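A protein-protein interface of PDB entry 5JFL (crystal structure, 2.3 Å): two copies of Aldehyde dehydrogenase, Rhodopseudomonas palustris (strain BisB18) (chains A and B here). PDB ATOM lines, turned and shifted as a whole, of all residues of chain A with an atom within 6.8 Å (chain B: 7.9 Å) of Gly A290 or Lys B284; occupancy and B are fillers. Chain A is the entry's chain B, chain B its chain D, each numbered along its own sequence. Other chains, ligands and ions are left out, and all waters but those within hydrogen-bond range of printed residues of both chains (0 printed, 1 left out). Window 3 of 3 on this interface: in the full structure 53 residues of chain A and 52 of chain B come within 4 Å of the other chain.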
ATOM      1  N   MET A 266       4.535  -5.541  22.161  1.00  0.00           N
ATOM      2  CA  MET A 266       4.391  -5.201  20.749  1.00  0.00           C
ATOM      3  C   MET A 266       3.230  -4.246  20.504  1.00  0.00           C
ATOM      4  O   MET A 266       3.233  -3.514  19.508  1.00  0.00           O
ATOM      5  CB  MET A 266       4.210  -6.476  19.930  1.00  0.00           C
ATOM      6  CG  MET A 266       5.338  -7.472  20.104  1.00  0.00           C
ATOM      7  SD  MET A 266       4.771  -9.168  19.933  1.00  0.00           S
ATOM      8  CE  MET A 266       4.746  -9.317  18.160  1.00  0.00           C
ATOM      9  N   ALA A 285       5.344 -12.084  13.683  1.00  0.00           N
ATOM     10  CA  ALA A 285       4.523 -11.414  14.683  1.00  0.00           C
ATOM     11  C   ALA A 285       4.976  -9.976  14.904  1.00  0.00           C
ATOM     12  O   ALA A 285       4.145  -9.065  14.997  1.00  0.00           O
ATOM     13  CB  ALA A 285       4.553 -12.199  15.994  1.00  0.00           C
ATOM     14  N   VAL A 286       6.290  -9.747  14.995  1.00  0.00           N
ATOM     15  CA  VAL A 286       6.772  -8.389  15.241  1.00  0.00           C
ATOM     16  C   VAL A 286       6.667  -7.538  13.981  1.00  0.00           C
ATOM     17  O   VAL A 286       6.575  -6.307  14.064  1.00  0.00           O
ATOM     18  CB  VAL A 286       8.213  -8.407  15.787  1.00  0.00           C
ATOM     19  CG1 VAL A 286       8.262  -9.091  17.145  1.00  0.00           C
ATOM     20  CG2 VAL A 286       9.157  -9.079  14.809  1.00  0.00           C
ATOM     21  N   LEU A 287       6.675  -8.164  12.805  1.00  0.00           N
ATOM     22  CA  LEU A 287       6.530  -7.438  11.550  1.00  0.00           C
ATOM     23  C   LEU A 287       5.078  -7.130  11.208  1.00  0.00           C
ATOM     24  O   LEU A 287       4.822  -6.518  10.164  1.00  0.00           O
ATOM     25  CB  LEU A 287       7.175  -8.225  10.407  1.00  0.00           C
ATOM     26  CG  LEU A 287       8.694  -8.398  10.467  1.00  0.00           C
ATOM     27  CD1 LEU A 287       9.163  -9.385   9.411  1.00  0.00           C
ATOM     28  CD2 LEU A 287       9.394  -7.057  10.298  1.00  0.00           C
ATOM     29  N   SER A 288       4.129  -7.538  12.051  1.00  0.00           N
ATOM     30  CA  SER A 288       2.714  -7.263  11.842  1.00  0.00           C
ATOM     31  C   SER A 288       2.166  -6.275  12.865  1.00  0.00           C
ATOM     32  O   SER A 288       0.951  -6.211  13.076  1.00  0.00           O
ATOM     33  CB  SER A 288       1.911  -8.564  11.883  1.00  0.00           C
ATOM     34  OG  SER A 288       2.497  -9.547  11.050  1.00  0.00           O
ATOM     35  N   THR A 289       3.041  -5.497  13.498  1.00  0.00           N
ATOM     36  CA  THR A 289       2.675  -4.640  14.615  1.00  0.00           C
ATOM     37  C   THR A 289       2.529  -3.174  14.232  1.00  0.00           C
ATOM     38  O   THR A 289       2.285  -2.342  15.112  1.00  0.00           O
ATOM     39  CB  THR A 289       3.718  -4.770  15.728  1.00  0.00           C
ATOM     40  OG1 THR A 289       5.024  -4.523  15.188  1.00  0.00           O
ATOM     41  CG2 THR A 289       3.682  -6.166  16.326  1.00  0.00           C
ATOM     42  N   GLY A 290       2.668  -2.835  12.952  1.00  0.00           N
ATOM     43  CA  GLY A 290       2.671  -1.443  12.558  1.00  0.00           C
ATOM     44  C   GLY A 290       3.872  -0.659  13.030  1.00  0.00           C
ATOM     45  O   GLY A 290       3.847   0.575  12.985  1.00  0.00           O
ATOM     46  N   LYS A 291       4.923  -1.339  13.484  1.00  0.00           N
ATOM     47  CA  LYS A 291       6.120  -0.696  14.001  1.00  0.00           C
ATOM     48  C   LYS A 291       7.348  -1.255  13.302  1.00  0.00           C
ATOM     49  O   LYS A 291       7.356  -2.403  12.850  1.00  0.00           O
ATOM     50  CB  LYS A 291       6.269  -0.905  15.514  1.00  0.00           C
ATOM     51  CG  LYS A 291       5.058  -0.514  16.334  1.00  0.00           C
ATOM     52  CD  LYS A 291       5.265  -0.874  17.792  1.00  0.00           C
ATOM     53  CE  LYS A 291       4.047  -0.526  18.625  1.00  0.00           C
ATOM     54  NZ  LYS A 291       3.735   0.927  18.563  1.00  0.00           N
ATOM     55  N   LYS A 292       8.382  -0.423  13.216  1.00  0.00           N
ATOM     56  CA  LYS A 292       9.699  -0.887  12.805  1.00  0.00           C
ATOM     57  C   LYS A 292      10.110  -2.086  13.646  1.00  0.00           C
ATOM     58  O   LYS A 292       9.952  -2.083  14.868  1.00  0.00           O
ATOM     59  CB  LYS A 292      10.715   0.247  12.960  1.00  0.00           C
ATOM     60  CG  LYS A 292      12.156  -0.153  12.721  1.00  0.00           C
ATOM     61  CD  LYS A 292      12.420  -0.390  11.251  1.00  0.00           C
ATOM     62  CE  LYS A 292      13.875  -0.746  11.014  1.00  0.00           C
ATOM     63  NZ  LYS A 292      14.175  -0.893   9.563  1.00  0.00           N
ATOM     64  N   MET B 266       0.596  -6.165  -0.696  1.00  0.00           N
ATOM     65  CA  MET B 266       1.077  -6.288   0.677  1.00  0.00           C
ATOM     66  C   MET B 266       0.923  -7.703   1.213  1.00  0.00           C
ATOM     67  O   MET B 266       1.656  -8.101   2.125  1.00  0.00           O
ATOM     68  CB  MET B 266       0.326  -5.320   1.590  1.00  0.00           C
ATOM     69  CG  MET B 266       0.598  -3.855   1.348  1.00  0.00           C
ATOM     70  SD  MET B 266      -0.250  -2.880   2.601  1.00  0.00           S
ATOM     71  CE  MET B 266       0.181  -1.226   2.095  1.00  0.00           C
ATOM     72  N   ALA B 276       7.105   2.087   1.190  1.00  0.00           N
ATOM     73  CA  ALA B 276       5.968   2.994   1.174  1.00  0.00           C
ATOM     74  C   ALA B 276       6.467   4.429   1.215  1.00  0.00           C
ATOM     75  O   ALA B 276       7.276   4.785   2.077  1.00  0.00           O
ATOM     76  CB  ALA B 276       5.031   2.725   2.352  1.00  0.00           C
ATOM     77  N   GLY B 278       4.488   7.791   1.301  1.00  0.00           N
ATOM     78  CA  GLY B 278       3.199   8.450   1.360  1.00  0.00           C
ATOM     79  C   GLY B 278       2.864   8.889   2.766  1.00  0.00           C
ATOM     80  O   GLY B 278       3.750   9.073   3.602  1.00  0.00           O
ATOM     81  N   GLY B 279       1.560   9.044   3.021  1.00  0.00           N
ATOM     82  CA  GLY B 279       1.093   9.576   4.270  1.00  0.00           C
ATOM     83  C   GLY B 279       1.279   8.606   5.423  1.00  0.00           C
ATOM     84  O   GLY B 279       1.837   7.512   5.271  1.00  0.00           O
ATOM     85  N   PRO B 280       0.806   9.008   6.607  1.00  0.00           N
ATOM     86  CA  PRO B 280       0.999   8.156   7.790  1.00  0.00           C
ATOM     87  C   PRO B 280       0.206   6.863   7.746  1.00  0.00           C
ATOM     88  O   PRO B 280       0.613   5.882   8.380  1.00  0.00           O
ATOM     89  CB  PRO B 280       0.549   9.059   8.948  1.00  0.00           C
ATOM     90  CG  PRO B 280      -0.394  10.032   8.321  1.00  0.00           C
ATOM     91  CD  PRO B 280       0.128  10.274   6.934  1.00  0.00           C
ATOM     92  N   ALA B 281      -0.913   6.825   7.016  1.00  0.00           N
ATOM     93  CA  ALA B 281      -1.729   5.616   6.988  1.00  0.00           C
ATOM     94  C   ALA B 281      -1.084   4.526   6.140  1.00  0.00           C
ATOM     95  O   ALA B 281      -1.113   3.348   6.511  1.00  0.00           O
ATOM     96  CB  ALA B 281      -3.131   5.939   6.474  1.00  0.00           C
ATOM     97  N   ILE B 282      -0.498   4.896   4.998  1.00  0.00           N
ATOM     98  CA  ILE B 282       0.129   3.897   4.139  1.00  0.00           C
ATOM     99  C   ILE B 282       1.389   3.341   4.796  1.00  0.00           C
ATOM    100  O   ILE B 282       1.700   2.151   4.665  1.00  0.00           O
ATOM    101  CB  ILE B 282       0.416   4.487   2.743  1.00  0.00           C
ATOM    102  CG1 ILE B 282       1.010   3.424   1.820  1.00  0.00           C
ATOM    103  CG2 ILE B 282       1.348   5.675   2.824  1.00  0.00           C
ATOM    104  CD1 ILE B 282       0.091   2.264   1.582  1.00  0.00           C
ATOM    105  N   VAL B 283       2.125   4.184   5.525  1.00  0.00           N
ATOM    106  CA  VAL B 283       3.307   3.710   6.236  1.00  0.00           C
ATOM    107  C   VAL B 283       2.905   2.826   7.409  1.00  0.00           C
ATOM    108  O   VAL B 283       3.619   1.876   7.755  1.00  0.00           O
ATOM    109  CB  VAL B 283       4.166   4.906   6.689  1.00  0.00           C
ATOM    110  CG1 VAL B 283       5.376   4.437   7.483  1.00  0.00           C
ATOM    111  CG2 VAL B 283       4.603   5.725   5.485  1.00  0.00           C
ATOM    112  N   LYS B 284       1.761   3.110   8.034  1.00  0.00           N
ATOM    113  CA  LYS B 284       1.270   2.254   9.106  1.00  0.00           C
ATOM    114  C   LYS B 284       0.880   0.877   8.583  1.00  0.00           C
ATOM    115  O   LYS B 284       0.984  -0.117   9.312  1.00  0.00           O
ATOM    116  CB  LYS B 284       0.081   2.921   9.801  1.00  0.00           C
ATOM    117  CG  LYS B 284      -0.449   2.181  11.020  1.00  0.00           C
ATOM    118  CD  LYS B 284       0.521   2.259  12.186  1.00  0.00           C
ATOM    119  CE  LYS B 284      -0.076   1.634  13.438  1.00  0.00           C
ATOM    120  NZ  LYS B 284       0.823   1.768  14.619  1.00  0.00           N
ATOM    121  N   ALA B 285       0.448   0.797   7.323  1.00  0.00           N
ATOM    122  CA  ALA B 285      -0.027  -0.470   6.775  1.00  0.00           C
ATOM    123  C   ALA B 285       1.133  -1.402   6.442  1.00  0.00           C
ATOM    124  O   ALA B 285       1.135  -2.570   6.846  1.00  0.00           O
ATOM    125  CB  ALA B 285      -0.889  -0.216   5.538  1.00  0.00           C
ATOM    126  N   VAL B 286       2.130  -0.900   5.706  1.00  0.00           N
ATOM    127  CA  VAL B 286       3.247  -1.734   5.268  1.00  0.00           C
ATOM    128  C   VAL B 286       4.008  -2.339   6.438  1.00  0.00           C
ATOM    129  O   VAL B 286       4.645  -3.386   6.283  1.00  0.00           O
ATOM    130  CB  VAL B 286       4.209  -0.928   4.370  1.00  0.00           C
ATOM    131  CG1 VAL B 286       3.551  -0.592   3.044  1.00  0.00           C
ATOM    132  CG2 VAL B 286       4.671   0.334   5.080  1.00  0.00           C
ATOM    133  N   LEU B 287       3.961  -1.708   7.608  1.00  0.00           N
ATOM    134  CA  LEU B 287       4.650  -2.201   8.793  1.00  0.00           C
ATOM    135  C   LEU B 287       3.817  -3.194   9.593  1.00  0.00           C
ATOM    136  O   LEU B 287       4.266  -3.649  10.651  1.00  0.00           O
ATOM    137  CB  LEU B 287       5.057  -1.026   9.683  1.00  0.00           C
ATOM    138  CG  LEU B 287       6.179  -0.172   9.094  1.00  0.00           C
ATOM    139  CD1 LEU B 287       6.432   1.067   9.938  1.00  0.00           C
ATOM    140  CD2 LEU B 287       7.445  -1.000   8.960  1.00  0.00           C
ATOM    141  N   SER B 288       2.623  -3.544   9.112  1.00  0.00           N
ATOM    142  CA  SER B 288       1.741  -4.486   9.791  1.00  0.00           C
ATOM    143  C   SER B 288       1.376  -5.670   8.903  1.00  0.00           C
ATOM    144  O   SER B 288       0.354  -6.324   9.138  1.00  0.00           O
ATOM    145  CB  SER B 288       0.476  -3.774  10.273  1.00  0.00           C
ATOM    146  OG  SER B 288      -0.160  -3.094   9.206  1.00  0.00           O
ATOM    147  N   THR B 289       2.194  -5.965   7.893  1.00  0.00           N
ATOM    148  CA  THR B 289       1.894  -7.005   6.919  1.00  0.00           C
ATOM    149  C   THR B 289       2.661  -8.299   7.153  1.00  0.00           C
ATOM    150  O   THR B 289       2.314  -9.321   6.553  1.00  0.00           O
ATOM    151  CB  THR B 289       2.194  -6.501   5.501  1.00  0.00           C
ATOM    152  OG1 THR B 289       3.565  -6.085   5.423  1.00  0.00           O
ATOM    153  CG2 THR B 289       1.294  -5.330   5.148  1.00  0.00           C
ATOM    154  N   GLY B 290       3.684  -8.286   8.002  1.00  0.00           N
ATOM    155  CA  GLY B 290       4.546  -9.436   8.160  1.00  0.00           C
ATOM    156  C   GLY B 290       5.740  -9.464   7.234  1.00  0.00           C
ATOM    157  O   GLY B 290       6.377 -10.516   7.102  1.00  0.00           O
ATOM    158  N   GLY B 295       9.332   2.612   5.463  1.00  0.00           N
ATOM    159  CA  GLY B 295       8.257   3.580   5.537  1.00  0.00           C
ATOM    160  C   GLY B 295       8.712   5.022   5.459  1.00  0.00           C
ATOM    161  O   GLY B 295       9.216   5.576   6.441  1.00  0.00           O
ATOM    162  N   GLY B 297       7.348   8.356   5.498  1.00  0.00           N
ATOM    163  CA  GLY B 297       6.119   9.020   5.874  1.00  0.00           C
ATOM    164  C   GLY B 297       6.104  10.495   5.532  1.00  0.00           C
ATOM    165  O   GLY B 297       6.905  10.992   4.737  1.00  0.00           O
ATOM    166  N   PRO B 498      10.693   7.116  10.299  1.00  0.00           N
ATOM    167  CA  PRO B 498      10.280   6.173  11.353  1.00  0.00           C
ATOM    168  C   PRO B 498      10.897   4.792  11.223  1.00  0.00           C
ATOM    169  O   PRO B 498      10.941   4.058  12.219  1.00  0.00           O
ATOM    170  CB  PRO B 498       8.753   6.121  11.199  1.00  0.00           C
ATOM    171  CG  PRO B 498       8.501   6.533   9.789  1.00  0.00           C
ATOM    172  CD  PRO B 498       9.545   7.566   9.493  1.00  0.00           C
ATOM    173  N   THR B 499      11.372   4.407  10.040  1.00  0.00           N
ATOM    174  CA  THR B 499      12.012   3.112   9.855  1.00  0.00           C
ATOM    175  C   THR B 499      13.532   3.208   9.766  1.00  0.00           C
ATOM    176  O   THR B 499      14.197   2.176   9.643  1.00  0.00           O
ATOM    177  CB  THR B 499      11.448   2.413   8.613  1.00  0.00           C
ATOM    178  OG1 THR B 499      11.551   3.281   7.477  1.00  0.00           O
ATOM    179  CG2 THR B 499       9.989   2.039   8.833  1.00  0.00           C
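O of Leu A287 is in hydrogen-bond range of N of Gly B290 (3.0 Å). The backbone NH (N) of Gly A290 is in hydrogen-bond range of the backbone carbonyl oxygen (O) of Leu B287 (2.9 Å). The side-chain amino group (NZ) of Lys A292 sits at hydrogen-bond distance from the backbone carbonyl oxygen (O) of Thr B499 (3.1 Å). O of Leu A287 lies close to O of Leu B287 (3.0 Å).
The side-chain hydroxyl (OG1) of Thr A289 is in hydrogen-bond range of the backbone carbonyl oxygen (O) of Val A286, 2.6 Å away. O of Lys B284 lies within hydrogen-bond range of OG of Ser B288, at 3.2 Å. The backbone carbonyl oxygen (O) of Ala B285 sits at hydrogen-bond distance from the side-chain hydroxyl (OG) of Ser B288, 2.7 Å away. The backbone carbonyl oxygen (O) of Val B286 is in hydrogen-bond range of the side-chain hydroxyl (OG1) of Thr B289, at 3.0 Å. OG1 of Thr B499 sits at hydrogen-bond distance from N of Gly B295.
Among the printed residues, merely in contact across the chains: Ser A288 with Gly B290 (3.5 Å), Leu A287 with Thr B289 (3.5 Å), Ser A288 with Ser B288 (3.6 Å), Gly A290 with Ser B288 (3.6 Å), Thr A289 with Leu B287 (3.6 Å), Gly A290 with Lys B284 (3.6 Å), Leu A287 with Ser B288 (3.7 Å), Lys A291 with Leu B287 (3.7 Å) and Lys A292 with Pro B498 (3.9 Å).
Met A266 touches none of the printed residues of chain B. Of the printed residues of chain B, Leu A287 touches Leu B287 (3.0 Å), Ser B288 (3.7 Å), Thr B289 (3.5 Å) and Gly B290 (3.0 Å). Printed residues of chain B within 4 Å of Lys A291: Leu B287 (3.7 Å). Printed residues of chain B within 4 Å of Lys A292: Pro B498 (3.9 Å) and Thr B499 (3.1 Å). Of chain A, only Gly A290 (3.6 Å) comes within 4 Å of Lys B284. Printed residues of chain A within 4 Å of Leu B287: Leu A287 (3.0 Å), Thr A289 (3.6 Å), Gly A290 (2.9 Å) and Lys A291 (3.7 Å). Of the printed residues of chain A, Gly B290 touches Leu A287 (3.0 Å) and Ser A288 (3.5 Å). Gly B295 touches none of the printed residues of chain A. The nearest printed residue of chain A that does not touch Ser B288 is Thr A289 (4.1 Å).
Of the 9 printed residues of chain A, 6 touch a printed residue of chain B. Hydrophobic or aromatic side chains of chain A within 4 Å of the printed part of chain B: Leu A287. Along chain A the printed residues that touch a printed residue of chain B span positions 287 to 292. Hydrophobic or aromatic side chains of chain B that line the printed part of chain A: Leu B287. Among the printed residues, no Asp or Glu carboxylate lies within 4 Å of a Lys or Arg side-chain nitrogen of the other chain.
Leu B287 touches its own counterpart, Leu A287. Leu A287 touches Thr B289, and with the chains exchanged Thr A289 touches Leu B287. Ser A288 touches its own counterpart, Ser B288. Ser A288 touches Gly B290, and with the chains exchanged Gly A290 touches Ser B288. Positions printed for both chains: 266, 285, 286, 287, 288, 289 and 290.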
